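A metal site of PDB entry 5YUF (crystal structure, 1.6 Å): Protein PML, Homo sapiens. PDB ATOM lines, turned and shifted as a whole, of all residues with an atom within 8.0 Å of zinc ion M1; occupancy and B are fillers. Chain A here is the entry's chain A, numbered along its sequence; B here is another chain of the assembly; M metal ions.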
ATOM      1  N   GLN A  10      25.345 -20.321 -17.193  1.00  0.00           N
ATOM      2  CA  GLN A  10      24.493 -20.107 -16.030  1.00  0.00           C
ATOM      3  C   GLN A  10      24.798 -21.069 -14.881  1.00  0.00           C
ATOM      4  O   GLN A  10      24.206 -20.932 -13.803  1.00  0.00           O
ATOM      5  CB  GLN A  10      23.022 -20.211 -16.408  1.00  0.00           C
ATOM      6  CG  GLN A  10      22.547 -19.123 -17.350  1.00  0.00           C
ATOM      7  CD  GLN A  10      21.103 -19.276 -17.745  1.00  0.00           C
ATOM      8  OE1 GLN A  10      20.737 -20.207 -18.457  1.00  0.00           O
ATOM      9  NE2 GLN A  10      20.274 -18.357 -17.285  1.00  0.00           N
ATOM     10  N   LEU A  22      19.465 -26.583 -25.304  1.00  0.00           N
ATOM     11  CA  LEU A  22      19.023 -27.596 -24.375  1.00  0.00           C
ATOM     12  C   LEU A  22      17.507 -27.624 -24.276  1.00  0.00           C
ATOM     13  O   LEU A  22      16.826 -26.662 -24.639  1.00  0.00           O
ATOM     14  CB  LEU A  22      19.623 -27.316 -22.997  1.00  0.00           C
ATOM     15  CG  LEU A  22      21.130 -27.048 -23.010  1.00  0.00           C
ATOM     16  CD1 LEU A  22      21.618 -26.749 -21.601  1.00  0.00           C
ATOM     17  CD2 LEU A  22      21.899 -28.222 -23.619  1.00  0.00           C
ATOM     18  N   PRO A  23      16.940 -28.715 -23.765  1.00  0.00           N
ATOM     19  CA  PRO A  23      15.471 -28.785 -23.682  1.00  0.00           C
ATOM     20  C   PRO A  23      14.864 -27.764 -22.728  1.00  0.00           C
ATOM     21  O   PRO A  23      13.749 -27.312 -22.980  1.00  0.00           O
ATOM     22  CB  PRO A  23      15.195 -30.222 -23.218  1.00  0.00           C
ATOM     23  CG  PRO A  23      16.509 -30.783 -22.797  1.00  0.00           C
ATOM     24  CD  PRO A  23      17.586 -30.001 -23.456  1.00  0.00           C
ATOM     25  N   CYS A  24      15.583 -27.406 -21.668  1.00  0.00           N
ATOM     26  CA  CYS A  24      15.158 -26.420 -20.669  1.00  0.00           C
ATOM     27  C   CYS A  24      15.474 -24.974 -21.006  1.00  0.00           C
ATOM     28  O   CYS A  24      15.027 -24.081 -20.287  1.00  0.00           O
ATOM     29  CB  CYS A  24      15.816 -26.755 -19.336  1.00  0.00           C
ATOM     30  SG  CYS A  24      17.610 -26.794 -19.457  1.00  0.00           S
ATOM     31  N   LEU A  25      16.260 -24.698 -22.045  1.00  0.00           N
ATOM     32  CA  LEU A  25      16.626 -23.308 -22.428  1.00  0.00           C
ATOM     33  C   LEU A  25      17.689 -22.665 -21.527  1.00  0.00           C
ATOM     34  O   LEU A  25      17.931 -21.457 -21.638  1.00  0.00           O
ATOM     35  CB  LEU A  25      15.382 -22.394 -22.456  1.00  0.00           C
ATOM     36  CG  LEU A  25      14.269 -22.835 -23.412  1.00  0.00           C
ATOM     37  CD1 LEU A  25      13.097 -21.885 -23.355  1.00  0.00           C
ATOM     38  CD2 LEU A  25      14.778 -22.926 -24.841  1.00  0.00           C
ATOM     39  N   HIS A  26      18.330 -23.415 -20.639  1.00  0.00           N
ATOM     40  CA  HIS A  26      19.470 -22.872 -19.914  1.00  0.00           C
ATOM     41  C   HIS A  26      20.682 -22.781 -20.840  1.00  0.00           C
ATOM     42  O   HIS A  26      20.772 -23.479 -21.865  1.00  0.00           O
ATOM     43  CB  HIS A  26      19.807 -23.713 -18.684  1.00  0.00           C
ATOM     44  CG  HIS A  26      18.911 -23.463 -17.511  1.00  0.00           C
ATOM     45  ND1 HIS A  26      18.170 -24.447 -16.901  1.00  0.00           N
ATOM     46  CD2 HIS A  26      18.652 -22.323 -16.828  1.00  0.00           C
ATOM     47  CE1 HIS A  26      17.483 -23.921 -15.906  1.00  0.00           C
ATOM     48  NE2 HIS A  26      17.752 -22.636 -15.845  1.00  0.00           N
ATOM     49  N   THR A  27      21.619 -21.912 -20.474  1.00  0.00           N
ATOM     50  CA  THR A  27      22.854 -21.701 -21.213  1.00  0.00           C
ATOM     51  C   THR A  27      24.001 -22.322 -20.422  1.00  0.00           C
ATOM     52  O   THR A  27      24.220 -21.956 -19.260  1.00  0.00           O
ATOM     53  CB  THR A  27      23.114 -20.213 -21.427  1.00  0.00           C
ATOM     54  OG1 THR A  27      22.046 -19.635 -22.171  1.00  0.00           O
ATOM     55  CG2 THR A  27      24.409 -19.995 -22.195  1.00  0.00           C
ATOM     56  N   LEU A  28      24.731 -23.262 -21.029  1.00  0.00           N
ATOM     57  CA  LEU A  28      25.851 -23.931 -20.382  1.00  0.00           C
ATOM     58  C   LEU A  28      27.109 -23.820 -21.230  1.00  0.00           C
ATOM     59  O   LEU A  28      27.036 -23.876 -22.455  1.00  0.00           O
ATOM     60  CB  LEU A  28      25.554 -25.403 -20.138  1.00  0.00           C
ATOM     61  CG  LEU A  28      24.350 -25.729 -19.262  1.00  0.00           C
ATOM     62  CD1 LEU A  28      24.150 -27.236 -19.163  1.00  0.00           C
ATOM     63  CD2 LEU A  28      24.503 -25.111 -17.892  1.00  0.00           C
ATOM     64  N   GLN A  39      21.253 -35.076 -17.176  1.00  0.00           N
ATOM     65  CA  GLN A  39      20.271 -34.057 -16.809  1.00  0.00           C
ATOM     66  C   GLN A  39      20.940 -32.703 -16.647  1.00  0.00           C
ATOM     67  O   GLN A  39      22.150 -32.610 -16.420  1.00  0.00           O
ATOM     68  CB  GLN A  39      19.530 -34.425 -15.513  1.00  0.00           C
ATOM     69  CG  GLN A  39      20.396 -34.331 -14.260  1.00  0.00           C
ATOM     70  CD  GLN A  39      19.815 -35.066 -13.071  1.00  0.00           C
ATOM     71  OE1 GLN A  39      18.836 -35.810 -13.191  1.00  0.00           O
ATOM     72  NE2 GLN A  39      20.393 -34.845 -11.907  1.00  0.00           N
ATOM     73  N   CYS A  40      20.134 -31.648 -16.735  1.00  0.00           N
ATOM     74  CA  CYS A  40      20.631 -30.287 -16.576  1.00  0.00           C
ATOM     75  C   CYS A  40      21.140 -30.078 -15.150  1.00  0.00           C
ATOM     76  O   CYS A  40      20.447 -30.438 -14.200  1.00  0.00           O
ATOM     77  CB  CYS A  40      19.548 -29.266 -16.894  1.00  0.00           C
ATOM     78  SG  CYS A  40      20.086 -27.535 -16.652  1.00  0.00           S
ATOM     79  N   PRO A  41      22.330 -29.480 -14.975  1.00  0.00           N
ATOM     80  CA  PRO A  41      22.813 -29.256 -13.596  1.00  0.00           C
ATOM     81  C   PRO A  41      22.065 -28.170 -12.864  1.00  0.00           C
ATOM     82  O   PRO A  41      22.176 -28.100 -11.639  1.00  0.00           O
ATOM     83  CB  PRO A  41      24.285 -28.864 -13.810  1.00  0.00           C
ATOM     84  CG  PRO A  41      24.315 -28.285 -15.191  1.00  0.00           C
ATOM     85  CD  PRO A  41      23.296 -29.052 -15.984  1.00  0.00           C
ATOM     86  N   ILE A  42      21.309 -27.333 -13.562  1.00  0.00           N
ATOM     87  CA  ILE A  42      20.538 -26.274 -12.908  1.00  0.00           C
ATOM     88  C   ILE A  42      19.135 -26.738 -12.543  1.00  0.00           C
ATOM     89  O   ILE A  42      18.722 -26.625 -11.377  1.00  0.00           O
ATOM     90  CB  ILE A  42      20.512 -25.015 -13.797  1.00  0.00           C
ATOM     91  CG1 ILE A  42      21.931 -24.563 -14.120  1.00  0.00           C
ATOM     92  CG2 ILE A  42      19.749 -23.888 -13.105  1.00  0.00           C
ATOM     93  CD1 ILE A  42      22.019 -23.511 -15.203  1.00  0.00           C
ATOM     94  N   CYS A  43      18.370 -27.266 -13.509  1.00  0.00           N
ATOM     95  CA  CYS A  43      16.967 -27.611 -13.302  1.00  0.00           C
ATOM     96  C   CYS A  43      16.676 -29.106 -13.378  1.00  0.00           C
ATOM     97  O   CYS A  43      15.537 -29.510 -13.122  1.00  0.00           O
ATOM     98  CB  CYS A  43      16.082 -26.896 -14.328  1.00  0.00           C
ATOM     99  SG  CYS A  43      16.332 -27.432 -16.058  1.00  0.00           S
ATOM    100  N   GLN A  44      17.653 -29.931 -13.752  1.00  0.00           N
ATOM    101  CA  GLN A  44      17.516 -31.380 -13.808  1.00  0.00           C
ATOM    102  C   GLN A  44      16.549 -31.847 -14.888  1.00  0.00           C
ATOM    103  O   GLN A  44      16.081 -32.988 -14.863  1.00  0.00           O
ATOM    104  CB  GLN A  44      17.116 -31.931 -12.440  1.00  0.00           C
ATOM    105  CG  GLN A  44      18.241 -31.795 -11.445  1.00  0.00           C
ATOM    106  CD  GLN A  44      17.979 -32.469 -10.119  1.00  0.00           C
ATOM    107  OE1 GLN A  44      16.878 -32.950  -9.853  1.00  0.00           O
ATOM    108  NE2 GLN A  44      19.005 -32.504  -9.277  1.00  0.00           N
ATOM    109  N   ALA A  45      16.255 -31.001 -15.864  1.00  0.00           N
ATOM    110  CA  ALA A  45      15.554 -31.475 -17.049  1.00  0.00           C
ATOM    111  C   ALA A  45      16.331 -32.639 -17.651  1.00  0.00           C
ATOM    112  O   ALA A  45      17.538 -32.520 -17.869  1.00  0.00           O
ATOM    113  CB  ALA A  45      15.415 -30.348 -18.075  1.00  0.00           C
ATOM    114  N   PRO A  46      15.692 -33.783 -17.905  1.00  0.00           N
ATOM    115  CA  PRO A  46      16.449 -34.920 -18.442  1.00  0.00           C
ATOM    116  C   PRO A  46      16.852 -34.709 -19.893  1.00  0.00           C
ATOM    117  O   PRO A  46      16.063 -34.261 -20.725  1.00  0.00           O
ATOM    118  CB  PRO A  46      15.477 -36.100 -18.302  1.00  0.00           C
ATOM    119  CG  PRO A  46      14.128 -35.517 -18.127  1.00  0.00           C
ATOM    120  CD  PRO A  46      14.288 -34.125 -17.607  1.00  0.00           C
ATOM    121  N   TRP A  47      18.088 -35.093 -20.207  1.00  0.00           N
ATOM    122  CA  TRP A  47      18.537 -35.072 -21.588  1.00  0.00           C
ATOM    123  C   TRP A  47      17.827 -36.173 -22.377  1.00  0.00           C
ATOM    124  O   TRP A  47      17.537 -37.236 -21.836  1.00  0.00           O
ATOM    125  CB  TRP A  47      20.044 -35.288 -21.682  1.00  0.00           C
ATOM    126  CG  TRP A  47      20.965 -34.248 -21.062  1.00  0.00           C
ATOM    127  CD1 TRP A  47      22.264 -34.467 -20.685  1.00  0.00           C
ATOM    128  CD2 TRP A  47      20.685 -32.874 -20.753  1.00  0.00           C
ATOM    129  NE1 TRP A  47      22.806 -33.316 -20.166  1.00  0.00           N
ATOM    130  CE2 TRP A  47      21.851 -32.322 -20.204  1.00  0.00           C
ATOM    131  CE3 TRP A  47      19.549 -32.060 -20.878  1.00  0.00           C
ATOM    132  CZ2 TRP A  47      21.941 -31.003 -19.777  1.00  0.00           C
ATOM    133  CZ3 TRP A  47      19.639 -30.741 -20.465  1.00  0.00           C
ATOM    134  CH2 TRP A  47      20.819 -30.228 -19.932  1.00  0.00           C
ATOM    135  N   PRO B  23      11.575 -23.787 -12.692  1.00  0.00           N
ATOM    136  CA  PRO B  23      13.027 -24.025 -12.567  1.00  0.00           C
ATOM    137  C   PRO B  23      13.708 -24.058 -13.912  1.00  0.00           C
ATOM    138  O   PRO B  23      14.882 -23.663 -14.027  1.00  0.00           O
ATOM    139  CB  PRO B  23      13.117 -25.381 -11.859  1.00  0.00           C
ATOM    140  CG  PRO B  23      11.751 -25.958 -11.888  1.00  0.00           C
ATOM    141  CD  PRO B  23      10.777 -24.851 -12.085  1.00  0.00           C
ATOM    142  N   CYS B  24      13.010 -24.538 -14.927  1.00  0.00           N
ATOM    143  CA  CYS B  24      13.420 -24.373 -16.295  1.00  0.00           C
ATOM    144  C   CYS B  24      12.949 -22.984 -16.711  1.00  0.00           C
ATOM    145  O   CYS B  24      12.231 -22.315 -15.972  1.00  0.00           O
ATOM    146  CB  CYS B  24      12.798 -25.455 -17.170  1.00  0.00           C
ATOM    147  SG  CYS B  24      10.993 -25.387 -17.132  1.00  0.00           S
ATOM    148  N   LEU B  25      13.338 -22.519 -17.884  1.00  0.00           N
ATOM    149  CA  LEU B  25      12.947 -21.143 -18.195  1.00  0.00           C
ATOM    150  C   LEU B  25      11.658 -21.052 -19.002  1.00  0.00           C
ATOM    151  O   LEU B  25      11.379 -20.000 -19.596  1.00  0.00           O
ATOM    152  CB  LEU B  25      14.116 -20.411 -18.879  1.00  0.00           C
ATOM    153  CG  LEU B  25      15.344 -20.356 -17.946  1.00  0.00           C
ATOM    154  CD1 LEU B  25      16.464 -19.517 -18.532  1.00  0.00           C
ATOM    155  CD2 LEU B  25      14.995 -19.848 -16.548  1.00  0.00           C
ATOM    156  N   CYS B  43       9.864 -29.907 -20.915  1.00  0.00           N
ATOM    157  CA  CYS B  43      11.203 -30.456 -20.742  1.00  0.00           C
ATOM    158  C   CYS B  43      11.310 -31.427 -19.589  1.00  0.00           C
ATOM    159  O   CYS B  43      12.381 -32.026 -19.412  1.00  0.00           O
ATOM    160  CB  CYS B  43      12.229 -29.331 -20.545  1.00  0.00           C
ATOM    161  SG  CYS B  43      12.078 -28.416 -18.967  1.00  0.00           S
ATOM    162  N   ALA B  45      11.648 -30.938 -16.472  1.00  0.00           N
ATOM    163  CA  ALA B  45      12.314 -30.486 -15.252  1.00  0.00           C
ATOM    164  C   ALA B  45      11.389 -30.696 -14.066  1.00  0.00           C
ATOM    165  O   ALA B  45      10.239 -30.229 -14.098  1.00  0.00           O
ATOM    166  CB  ALA B  45      12.707 -29.015 -15.370  1.00  0.00           C
HETATM  167 ZN    ZN M   1      18.097 -26.477 -17.233  1.00  0.00          ZN
HETATM  168 ZN    ZN M   2      10.420 -26.719 -18.931  1.00  0.00          ZN
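O of Cys 24 of chain A is in hydrogen-bond range of N of Leu 25 of chain B (3.3 Å). The backbone NH (N) of Cys 40 sits at hydrogen-bond distance from the backbone carbonyl oxygen (O) of Ala 45 of chain A, at 3.0 Å. The side-chain sulfur of Cys 43 of chain A lies close to the backbone NH of Ala 45 of chain A (3.6 Å). The side-chain sulfur (SG) of Cys 40 sits close to the backbone NH (N) of Ile 42, at 3.3 Å.
Four residues have an atom within 4 Å of zinc ion M1: Cys 24 of chain A, His 26, Cys 40 and Cys 43 of chain A.
Zinc ion M1 is bound by a ring nitrogen (ND1) of His 26 (2.1 Å), the side-chain sulfur (SG) of Cys 24 of chain A (2.3 Å), the side-chain sulfur (SG) of Cys 43 of chain A (2.3 Å) and the side-chain sulfur (SG) of Cys 40 (2.3 Å).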
